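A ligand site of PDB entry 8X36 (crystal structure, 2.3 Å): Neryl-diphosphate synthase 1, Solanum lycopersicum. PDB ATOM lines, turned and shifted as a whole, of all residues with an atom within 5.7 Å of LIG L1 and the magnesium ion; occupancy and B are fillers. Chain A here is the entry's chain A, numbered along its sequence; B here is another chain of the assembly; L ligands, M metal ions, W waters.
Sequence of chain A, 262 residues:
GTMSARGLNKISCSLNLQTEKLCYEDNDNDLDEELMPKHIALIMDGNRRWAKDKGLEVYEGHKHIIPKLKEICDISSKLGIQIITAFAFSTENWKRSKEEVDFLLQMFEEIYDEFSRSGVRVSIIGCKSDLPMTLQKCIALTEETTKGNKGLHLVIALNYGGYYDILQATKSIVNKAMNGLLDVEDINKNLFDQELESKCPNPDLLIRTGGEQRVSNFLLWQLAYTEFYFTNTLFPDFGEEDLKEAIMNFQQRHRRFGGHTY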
ATOM      1  N   ILE A  43       2.361  18.122  17.241  1.00  0.00           N
ATOM      2  CA  ILE A  43       1.041  17.497  17.285  1.00  0.00           C
ATOM      3  C   ILE A  43       0.163  18.147  16.225  1.00  0.00           C
ATOM      4  O   ILE A  43      -0.252  19.299  16.405  1.00  0.00           O
ATOM      5  CB  ILE A  43       0.390  17.600  18.664  1.00  0.00           C
ATOM      6  CG1 ILE A  43       1.222  16.869  19.732  1.00  0.00           C
ATOM      7  CG2 ILE A  43      -1.071  17.119  18.588  1.00  0.00           C
ATOM      8  CD1 ILE A  43       0.677  16.992  21.154  1.00  0.00           C
ATOM      9  N   MET A  44      -0.139  17.414  15.150  1.00  0.00           N
ATOM     10  CA  MET A  44      -0.744  17.967  13.925  1.00  0.00           C
ATOM     11  C   MET A  44      -2.261  17.883  14.007  1.00  0.00           C
ATOM     12  O   MET A  44      -2.892  17.090  13.330  1.00  0.00           O
ATOM     13  CB  MET A  44      -0.242  17.197  12.685  1.00  0.00           C
ATOM     14  CG  MET A  44       1.225  16.828  12.737  1.00  0.00           C
ATOM     15  SD  MET A  44       1.884  16.094  11.222  1.00  0.00           S
ATOM     16  CE  MET A  44       1.582  14.361  11.539  1.00  0.00           C
ATOM     17  N   ASP A  45      -2.845  18.729  14.850  1.00  0.00           N
ATOM     18  CA  ASP A  45      -4.268  18.701  15.175  1.00  0.00           C
ATOM     19  C   ASP A  45      -4.990  19.800  14.396  1.00  0.00           C
ATOM     20  O   ASP A  45      -4.393  20.830  14.050  1.00  0.00           O
ATOM     21  CB  ASP A  45      -4.480  18.885  16.684  1.00  0.00           C
ATOM     22  CG  ASP A  45      -5.891  18.539  17.148  1.00  0.00           C
ATOM     23  OD1 ASP A  45      -6.543  17.710  16.485  1.00  0.00           O
ATOM     24  OD2 ASP A  45      -6.338  19.088  18.189  1.00  0.00           O
ATOM     25  N   GLY A  46      -6.268  19.579  14.126  1.00  0.00           N
ATOM     26  CA  GLY A  46      -7.152  20.592  13.580  1.00  0.00           C
ATOM     27  C   GLY A  46      -7.653  20.331  12.158  1.00  0.00           C
ATOM     28  O   GLY A  46      -8.225  21.247  11.543  1.00  0.00           O
ATOM     29  N   ARG A  48     -10.044  18.216  10.757  1.00  0.00           N
ATOM     30  CA  ARG A  48     -11.467  18.120  10.453  1.00  0.00           C
ATOM     31  C   ARG A  48     -12.140  19.497  10.487  1.00  0.00           C
ATOM     32  O   ARG A  48     -12.866  19.868   9.560  1.00  0.00           O
ATOM     33  CB  ARG A  48     -12.160  17.128  11.411  1.00  0.00           C
ATOM     34  CG  ARG A  48     -11.401  15.790  11.505  1.00  0.00           C
ATOM     35  CD  ARG A  48     -12.171  14.593  12.154  1.00  0.00           C
ATOM     36  NE  ARG A  48     -12.349  14.745  13.594  1.00  0.00           N
ATOM     37  CZ  ARG A  48     -12.757  13.796  14.432  1.00  0.00           C
ATOM     38  NH1 ARG A  48     -13.003  12.560  14.014  1.00  0.00           N
ATOM     39  NH2 ARG A  48     -12.926  14.090  15.715  1.00  0.00           N
ATOM     40  N   ARG A  49     -11.882  20.288  11.549  1.00  0.00           N
ATOM     41  CA  ARG A  49     -12.460  21.628  11.636  1.00  0.00           C
ATOM     42  C   ARG A  49     -12.009  22.511  10.476  1.00  0.00           C
ATOM     43  O   ARG A  49     -12.765  23.367  10.019  1.00  0.00           O
ATOM     44  CB  ARG A  49     -12.104  22.298  12.971  1.00  0.00           C
ATOM     45  CG  ARG A  49     -12.778  21.666  14.198  1.00  0.00           C
ATOM     46  CD  ARG A  49     -12.028  21.997  15.517  1.00  0.00           C
ATOM     47  NE  ARG A  49     -10.804  21.227  15.740  1.00  0.00           N
ATOM     48  CZ  ARG A  49      -9.867  21.576  16.626  1.00  0.00           C
ATOM     49  NH1 ARG A  49      -9.953  22.700  17.316  1.00  0.00           N
ATOM     50  NH2 ARG A  49      -8.839  20.755  16.845  1.00  0.00           N
ATOM     51  N   PHE A  87       3.110  13.603  15.441  1.00  0.00           N
ATOM     52  CA  PHE A  87       2.050  12.709  15.876  1.00  0.00           C
ATOM     53  C   PHE A  87       1.050  12.554  14.729  1.00  0.00           C
ATOM     54  O   PHE A  87       0.342  13.512  14.398  1.00  0.00           O
ATOM     55  CB  PHE A  87       1.415  13.262  17.144  1.00  0.00           C
ATOM     56  CG  PHE A  87       0.841  12.223  18.099  1.00  0.00           C
ATOM     57  CD1 PHE A  87       1.098  10.872  17.926  1.00  0.00           C
ATOM     58  CD2 PHE A  87       0.132  12.636  19.223  1.00  0.00           C
ATOM     59  CE1 PHE A  87       0.589   9.930  18.832  1.00  0.00           C
ATOM     60  CE2 PHE A  87      -0.378  11.714  20.156  1.00  0.00           C
ATOM     61  CZ  PHE A  87      -0.151  10.360  19.976  1.00  0.00           C
ATOM     62  N   ALA A  88       1.025  11.392  14.084  1.00  0.00           N
ATOM     63  CA  ALA A  88       0.154  11.191  12.927  1.00  0.00           C
ATOM     64  C   ALA A  88      -1.093  10.370  13.246  1.00  0.00           C
ATOM     65  O   ALA A  88      -2.116  10.547  12.576  1.00  0.00           O
ATOM     66  CB  ALA A  88       0.907  10.497  11.773  1.00  0.00           C
ATOM     67  N   PHE A  89      -1.025   9.479  14.239  1.00  0.00           N
ATOM     68  CA  PHE A  89      -2.141   8.599  14.572  1.00  0.00           C
ATOM     69  C   PHE A  89      -1.850   8.036  15.954  1.00  0.00           C
ATOM     70  O   PHE A  89      -0.773   7.473  16.157  1.00  0.00           O
ATOM     71  CB  PHE A  89      -2.251   7.468  13.530  1.00  0.00           C
ATOM     72  CG  PHE A  89      -3.545   6.692  13.595  1.00  0.00           C
ATOM     73  CD1 PHE A  89      -4.695   7.142  12.947  1.00  0.00           C
ATOM     74  CD2 PHE A  89      -3.603   5.515  14.328  1.00  0.00           C
ATOM     75  CE1 PHE A  89      -5.895   6.402  13.016  1.00  0.00           C
ATOM     76  CE2 PHE A  89      -4.785   4.783  14.399  1.00  0.00           C
ATOM     77  CZ  PHE A  89      -5.932   5.224  13.754  1.00  0.00           C
ATOM     78  N   SER A  90      -2.766   8.243  16.918  1.00  0.00           N
ATOM     79  CA  SER A  90      -2.568   7.776  18.287  1.00  0.00           C
ATOM     80  C   SER A  90      -3.288   6.451  18.514  1.00  0.00           C
ATOM     81  O   SER A  90      -4.196   6.089  17.764  1.00  0.00           O
ATOM     82  CB  SER A  90      -3.071   8.816  19.295  1.00  0.00           C
ATOM     83  OG  SER A  90      -4.484   8.746  19.442  1.00  0.00           O
ATOM     84  N   ASN A  93      -7.051   6.849  18.401  1.00  0.00           N
ATOM     85  CA  ASN A  93      -7.792   7.218  17.207  1.00  0.00           C
ATOM     86  C   ASN A  93      -8.534   6.037  16.592  1.00  0.00           C
ATOM     87  O   ASN A  93      -9.377   6.248  15.716  1.00  0.00           O
ATOM     88  CB  ASN A  93      -6.867   7.884  16.181  1.00  0.00           C
ATOM     89  CG  ASN A  93      -6.372   9.264  16.657  1.00  0.00           C
ATOM     90  OD1 ASN A  93      -5.266   9.694  16.321  1.00  0.00           O
ATOM     91  ND2 ASN A  93      -7.198   9.948  17.447  1.00  0.00           N
ATOM     92  N   ARG A  96     -12.513   6.320  16.191  1.00  0.00           N
ATOM     93  CA  ARG A  96     -13.281   7.012  15.168  1.00  0.00           C
ATOM     94  C   ARG A  96     -13.986   5.963  14.300  1.00  0.00           C
ATOM     95  O   ARG A  96     -13.893   4.758  14.528  1.00  0.00           O
ATOM     96  CB  ARG A  96     -12.363   7.945  14.395  1.00  0.00           C
ATOM     97  CG  ARG A  96     -11.731   8.965  15.326  1.00  0.00           C
ATOM     98  CD  ARG A  96     -10.648   9.768  14.686  1.00  0.00           C
ATOM     99  NE  ARG A  96     -10.146  10.796  15.583  1.00  0.00           N
ATOM    100  CZ  ARG A  96      -9.547  11.914  15.196  1.00  0.00           C
ATOM    101  NH1 ARG A  96      -9.368  12.180  13.912  1.00  0.00           N
ATOM    102  NH2 ARG A  96      -9.124  12.785  16.110  1.00  0.00           N
ATOM    103  N   ARG A 208       1.786  22.413  19.314  1.00  0.00           N
ATOM    104  CA  ARG A 208       0.484  21.829  19.048  1.00  0.00           C
ATOM    105  C   ARG A 208      -0.408  22.853  18.372  1.00  0.00           C
ATOM    106  O   ARG A 208      -0.756  23.870  18.990  1.00  0.00           O
ATOM    107  CB  ARG A 208      -0.204  21.300  20.300  1.00  0.00           C
ATOM    108  CG  ARG A 208      -1.671  20.883  20.018  1.00  0.00           C
ATOM    109  CD  ARG A 208      -2.286  20.016  21.135  1.00  0.00           C
ATOM    110  NE  ARG A 208      -3.486  19.336  20.662  1.00  0.00           N
ATOM    111  CZ  ARG A 208      -3.947  18.189  21.153  1.00  0.00           C
ATOM    112  NH1 ARG A 208      -3.329  17.579  22.151  1.00  0.00           N
ATOM    113  NH2 ARG A 208      -5.038  17.639  20.613  1.00  0.00           N
ATOM    114  N   GLU A 212      -6.121  23.269  21.198  1.00  0.00           N
ATOM    115  CA  GLU A 212      -6.356  22.566  22.464  1.00  0.00           C
ATOM    116  C   GLU A 212      -5.073  22.547  23.298  1.00  0.00           C
ATOM    117  O   GLU A 212      -3.967  22.469  22.763  1.00  0.00           O
ATOM    118  CB  GLU A 212      -6.844  21.141  22.221  1.00  0.00           C
ATOM    119  CG  GLU A 212      -7.873  21.041  21.108  1.00  0.00           C
ATOM    120  CD  GLU A 212      -9.263  21.438  21.574  1.00  0.00           C
ATOM    121  OE1 GLU A 212      -9.457  21.596  22.809  1.00  0.00           O
ATOM    122  OE2 GLU A 212     -10.161  21.615  20.723  1.00  0.00           O
ATOM    123  N   ARG A 214      -3.304  20.379  25.824  1.00  0.00           N
ATOM    124  CA  ARG A 214      -3.209  19.012  26.343  1.00  0.00           C
ATOM    125  C   ARG A 214      -2.260  18.263  25.419  1.00  0.00           C
ATOM    126  O   ARG A 214      -2.026  18.684  24.281  1.00  0.00           O
ATOM    127  CB  ARG A 214      -4.575  18.338  26.388  1.00  0.00           C
ATOM    128  CG  ARG A 214      -5.444  18.538  25.128  1.00  0.00           C
ATOM    129  CD  ARG A 214      -6.664  17.611  25.192  1.00  0.00           C
ATOM    130  NE  ARG A 214      -7.495  17.621  23.986  1.00  0.00           N
ATOM    131  CZ  ARG A 214      -8.679  18.222  23.885  1.00  0.00           C
ATOM    132  NH1 ARG A 214      -9.153  18.994  24.857  1.00  0.00           N
ATOM    133  NH2 ARG A 214      -9.407  18.056  22.775  1.00  0.00           N
ATOM    134  N   SER A 216      -2.518  14.725  24.877  1.00  0.00           N
ATOM    135  CA  SER A 216      -3.225  13.596  24.249  1.00  0.00           C
ATOM    136  C   SER A 216      -2.348  12.335  24.132  1.00  0.00           C
ATOM    137  O   SER A 216      -2.236  11.733  23.065  1.00  0.00           O
ATOM    138  CB  SER A 216      -3.772  14.011  22.870  1.00  0.00           C
ATOM    139  OG  SER A 216      -4.611  15.159  22.969  1.00  0.00           O
ATOM    140  N   TYR B 225      -4.143  12.937  29.273  1.00  0.00           N
ATOM    141  CA  TYR B 225      -5.264  13.705  28.717  1.00  0.00           C
ATOM    142  C   TYR B 225      -5.746  14.828  29.648  1.00  0.00           C
ATOM    143  O   TYR B 225      -6.893  15.263  29.542  1.00  0.00           O
ATOM    144  CB  TYR B 225      -6.408  12.758  28.320  1.00  0.00           C
ATOM    145  CG  TYR B 225      -6.153  12.000  27.017  1.00  0.00           C
ATOM    146  CD1 TYR B 225      -6.492  12.572  25.789  1.00  0.00           C
ATOM    147  CD2 TYR B 225      -5.560  10.726  27.014  1.00  0.00           C
ATOM    148  CE1 TYR B 225      -6.259  11.907  24.597  1.00  0.00           C
ATOM    149  CE2 TYR B 225      -5.321  10.050  25.815  1.00  0.00           C
ATOM    150  CZ  TYR B 225      -5.665  10.650  24.611  1.00  0.00           C
ATOM    151  OH  TYR B 225      -5.434  10.024  23.398  1.00  0.00           O
ATOM    152  N   HIS B 254     -13.528  21.419  25.276  1.00  0.00           N
ATOM    153  CA  HIS B 254     -14.116  20.220  24.704  1.00  0.00           C
ATOM    154  C   HIS B 254     -13.070  19.108  24.657  1.00  0.00           C
ATOM    155  O   HIS B 254     -12.057  19.209  23.952  1.00  0.00           O
ATOM    156  CB  HIS B 254     -14.662  20.483  23.307  1.00  0.00           C
ATOM    157  CG  HIS B 254     -15.536  21.697  23.235  1.00  0.00           C
ATOM    158  ND1 HIS B 254     -16.899  21.630  23.403  1.00  0.00           N
ATOM    159  CD2 HIS B 254     -15.238  23.000  23.037  1.00  0.00           C
ATOM    160  CE1 HIS B 254     -17.409  22.846  23.303  1.00  0.00           C
ATOM    161  NE2 HIS B 254     -16.426  23.692  23.083  1.00  0.00           N
ATOM    162  N   ARG B 255     -13.348  18.035  25.407  1.00  0.00           N
ATOM    163  CA  ARG B 255     -12.451  16.910  25.591  1.00  0.00           C
ATOM    164  C   ARG B 255     -12.934  15.745  24.730  1.00  0.00           C
ATOM    165  O   ARG B 255     -14.080  15.300  24.860  1.00  0.00           O
ATOM    166  CB  ARG B 255     -12.432  16.516  27.079  1.00  0.00           C
ATOM    167  CG  ARG B 255     -12.026  17.660  28.000  1.00  0.00           C
ATOM    168  CD  ARG B 255     -11.893  17.235  29.470  1.00  0.00           C
ATOM    169  NE  ARG B 255     -10.656  16.516  29.769  1.00  0.00           N
ATOM    170  CZ  ARG B 255     -10.456  15.797  30.871  1.00  0.00           C
ATOM    171  NH1 ARG B 255     -11.397  15.676  31.809  1.00  0.00           N
ATOM    172  NH2 ARG B 255      -9.297  15.176  31.044  1.00  0.00           N
ATOM    173  N   ARG B 256     -12.075  15.258  23.828  1.00  0.00           N
ATOM    174  CA  ARG B 256     -12.464  14.207  22.901  1.00  0.00           C
ATOM    175  C   ARG B 256     -11.800  12.852  23.155  1.00  0.00           C
ATOM    176  O   ARG B 256     -12.345  11.833  22.751  1.00  0.00           O
ATOM    177  CB  ARG B 256     -12.219  14.663  21.441  1.00  0.00           C
ATOM    178  CG  ARG B 256     -13.113  15.904  21.062  1.00  0.00           C
ATOM    179  CD  ARG B 256     -12.995  16.403  19.604  1.00  0.00           C
ATOM    180  NE  ARG B 256     -11.932  17.375  19.375  1.00  0.00           N
ATOM    181  CZ  ARG B 256     -11.994  18.672  19.639  1.00  0.00           C
ATOM    182  NH1 ARG B 256     -13.086  19.226  20.152  1.00  0.00           N
ATOM    183  NH2 ARG B 256     -10.945  19.450  19.377  1.00  0.00           N
ATOM    184  N   PHE B 257     -10.662  12.831  23.869  1.00  0.00           N
ATOM    185  CA  PHE B 257      -9.991  11.575  24.250  1.00  0.00           C
ATOM    186  C   PHE B 257      -9.685  10.723  23.013  1.00  0.00           C
ATOM    187  O   PHE B 257      -9.837   9.496  23.038  1.00  0.00           O
ATOM    188  CB  PHE B 257     -10.819  10.778  25.277  1.00  0.00           C
ATOM    189  CG  PHE B 257     -11.191  11.558  26.504  1.00  0.00           C
ATOM    190  CD1 PHE B 257     -10.257  11.820  27.504  1.00  0.00           C
ATOM    191  CD2 PHE B 257     -12.488  12.047  26.665  1.00  0.00           C
ATOM    192  CE1 PHE B 257     -10.601  12.560  28.642  1.00  0.00           C
ATOM    193  CE2 PHE B 257     -12.843  12.785  27.811  1.00  0.00           C
ATOM    194  CZ  PHE B 257     -11.901  13.034  28.795  1.00  0.00           C
ATOM    195  N   GLY B 258      -9.262  11.383  21.919  1.00  0.00           N
ATOM    196  CA  GLY B 258      -8.907  10.699  20.697  1.00  0.00           C
ATOM    197  C   GLY B 258     -10.068  10.377  19.772  1.00  0.00           C
ATOM    198  O   GLY B 258      -9.836   9.992  18.619  1.00  0.00           O
ATOM    199  N   GLY B 259     -11.308  10.553  20.209  1.00  0.00           N
ATOM    200  CA  GLY B 259     -12.483  10.203  19.455  1.00  0.00           C
ATOM    201  C   GLY B 259     -13.178  11.394  18.831  1.00  0.00           C
ATOM    202  O   GLY B 259     -12.572  12.459  18.616  1.00  0.00           O
HETATM  203  C1  LIG L   1      -3.980  13.999  18.771  1.00  0.00           C
HETATM  204  O1  LIG L   1      -5.110  14.589  18.190  1.00  0.00           O
HETATM  205  C2  LIG L   1      -3.592  12.722  18.022  1.00  0.00           C
HETATM  206  C3  LIG L   1      -2.945  13.044  16.659  1.00  0.00           C
HETATM  207  C4  LIG L   1      -2.748  12.065  15.774  1.00  0.00           C
HETATM  208  C5  LIG L   1      -2.516  14.481  16.315  1.00  0.00           C
HETATM  209  P1  LIG L   1      -6.587  14.262  18.824  1.00  0.00           P
HETATM  210  O2  LIG L   1      -7.688  14.999  18.079  1.00  0.00           O
HETATM  211  O3  LIG L   1      -6.832  12.764  18.836  1.00  0.00           O
HETATM  212  O4  LIG L   1      -6.546  14.742  20.379  1.00  0.00           O
HETATM  213  P2  LIG L   1      -7.799  15.092  21.374  1.00  0.00           P
HETATM  214  O5  LIG L   1      -8.918  14.089  21.260  1.00  0.00           O
HETATM  215  O6  LIG L   1      -8.340  16.466  21.040  1.00  0.00           O
HETATM  216  O7  LIG L   1      -7.201  15.029  22.748  1.00  0.00           O
HETATM  217  O1  LG2 L   2     -10.383  19.354  13.998  1.00  0.00           O
HETATM  218  P1  LG2 L   2     -10.069  17.946  14.485  1.00  0.00           P
HETATM  219  O2  LG2 L   2     -11.321  17.134  14.737  1.00  0.00           O
HETATM  220  O3  LG2 L   2      -9.266  18.029  15.769  1.00  0.00           O
HETATM  221  O4  LG2 L   2      -9.128  17.208  13.365  1.00  0.00           O
HETATM  222  P2  LG2 L   2      -8.218  15.873  13.675  1.00  0.00           P
HETATM  223  O5  LG2 L   2      -8.401  15.433  15.114  1.00  0.00           O
HETATM  224  O6  LG2 L   2      -8.635  14.708  12.809  1.00  0.00           O
HETATM  225  S1  LG2 L   2      -6.214  16.378  13.413  1.00  0.00           S
HETATM  226  C1  LG2 L   2      -5.265  15.220  14.440  1.00  0.00           C
HETATM  227  C2  LG2 L   2      -5.680  13.817  14.010  1.00  0.00           C
HETATM  228  C3  LG2 L   2      -4.910  13.159  13.158  1.00  0.00           C
HETATM  229  C4  LG2 L   2      -5.291  11.761  12.703  1.00  0.00           C
HETATM  230  C5  LG2 L   2      -3.631  13.811  12.654  1.00  0.00           C
HETATM  231 MG    MG M   1      -8.044  16.632  17.023  1.00  0.00          MG
HETATM  232  O   HOH W   1      -8.330  17.792  18.816  1.00  0.00           O
HETATM  233  O   HOH W   2      -5.363  11.039  20.448  1.00  0.00           O
HETATM  234  O   HOH W   3     -10.331  13.551  18.804  1.00  0.00           O
HETATM  235  O   HOH W   4      -9.070  15.267  24.896  1.00  0.00           O
HETATM  236  O   HOH W   5     -10.044  15.834  17.269  1.00  0.00           O
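The backbone NH of Gly 46 sits close to a sulfur (S1) of LG2 L2 (3.3 Å). The backbone NH (N) of Phe 257 of chain B lies within hydrogen-bond range of an oxygen (O5) of LIG L1, at 3.4 Å. The guanidinium group of Arg 214 lies within salt-bridge range of an oxygen (O6) of LIG L1, at 2.6 Å. NE of Arg 48 is in salt-bridge range of O2 of LG2 L2 (2.8 Å). The backbone NH (N) of Arg 48 lies within hydrogen-bond range of an oxygen (O4) of LG2 L2, 2.9 Å away. The guanidinium group (NH2) of Arg 208 is in salt-bridge range of an oxygen (O6) of LIG L1 (3.5 Å). The guanidinium group (NE) of Arg 49 is in salt-bridge range of an oxygen (O1) of LG2 L2 (2.6 Å). The side-chain hydroxyl (OG) of Ser 216 sits at hydrogen-bond distance from an oxygen (O7) of LIG L1 (2.6 Å). An oxygen (O3) of LIG L1 lies within salt-bridge range of the guanidinium group (NH2) of Arg 96. O6 of LG2 L2 lies within salt-bridge range of NH1 of Arg 96, 2.9 Å away. The backbone NH of Arg 49 is in hydrogen-bond range of an oxygen (O1) of LG2 L2 (3.0 Å). The backbone NH (N) of Gly 258 of chain B is in hydrogen-bond range of an oxygen (O5) of LIG L1, at 2.8 Å. ND2 of Asn 93 lies within hydrogen-bond range of O3 of LIG L1 (3.2 Å).
The guanidinium group (NH1) of Arg 208 is in hydrogen-bond range of the side-chain hydroxyl (OG) of Ser 216, at 2.9 Å. O of Gly 258 of chain B lies within hydrogen-bond range of ND2 of Asn 93, 2.9 Å away. The guanidinium group of Arg 256 of chain B is in salt-bridge range of the side-chain carboxylate of Glu 212 (2.7 Å). The guanidinium group of Arg 255 of chain B is in hydrogen-bond range of the backbone carbonyl oxygen of Tyr 225 of chain B, 2.8 Å away. The guanidinium group (NH1) of Arg 208 lies within hydrogen-bond range of the backbone carbonyl oxygen (O) of Arg 214, 2.7 Å away. The side-chain carboxylate (OE1) of Glu 212 is in salt-bridge range of the guanidinium group (NH1) of Arg 214. NE of Arg 96 is in hydrogen-bond range of O of Gly 258 of chain B (3.2 Å). The side-chain carboxylate (OD2) of Asp 45 lies within salt-bridge range of the guanidinium group (NH2) of Arg 49, at 3.3 Å.
CG2 of Ile 43 touches C5 of LIG L1, 3.8 Å away. N of Met 44 touches C5 of LIG L1, at 3.95 Å. O of Phe 87 touches C5 of LIG L1, at 3.6 Å. Ala 88 touches LIG L1 (C to C4, 3.5 Å). Phe 89 touches LIG L1 (N to C4, 3.5 Å). Ser 90 touches LIG L1 (N to C4, 3.99 Å). Tyr 225 of chain B touches LIG L1 (CE1 to O7, 3.7 Å). CB of Arg 256 of chain B touches O5 of LIG L1 (3.4 Å). Hydrophobic or aromatic side chains that line LIG L1: Ile 43, Phe 87 and Tyr 225 of chain B. The nearest printed residue that does not touch LIG L1 is Gly 259 of chain B (4.4 Å).
Of the 23 residues printed, 1 comes within 4 Å of the magnesium ion. The nearest printed residue that does not touch the magnesium ion is Arg 96 (4.1 Å).
The magnesium ion is bound by OD1 of Asp 45, at 1.9 Å. The magnesium ion is bound by O2 of LIG L1 (2.0 Å). Water W1 binds the magnesium ion, at 2.2 Å. The magnesium ion is bound by water W5. O3 of LG2 L2 is bound to the magnesium ion (2.2 Å). O5 of LG2 L2 binds the magnesium ion, at 2.3 Å. The magnesium ion has six donor atoms within binding distance.
Water W1 lies within hydrogen-bond range of OD2 of Asp 45 (2.5 Å), O6 of LIG L1 (2.6 Å) and NH2 of Arg 256 of chain B (3.1 Å). Water W5 lies within hydrogen-bond range of O2 of LG2 L2, NE of Arg 256 of chain B and NH2 of Arg 96. Water W2 lies within hydrogen-bond range of the side-chain hydroxyl (OG) of Ser 90, an oxygen (O3) of LIG L1 and the side-chain hydroxyl (OH) of Tyr 225 of chain B. Water W3 lies within hydrogen-bond range of the backbone carbonyl oxygen (O) of Gly 259 of chain B (2.5 Å), an oxygen (O5) of LIG L1 (2.9 Å) and the guanidinium group (NH2) of Arg 96 (3.0 Å).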
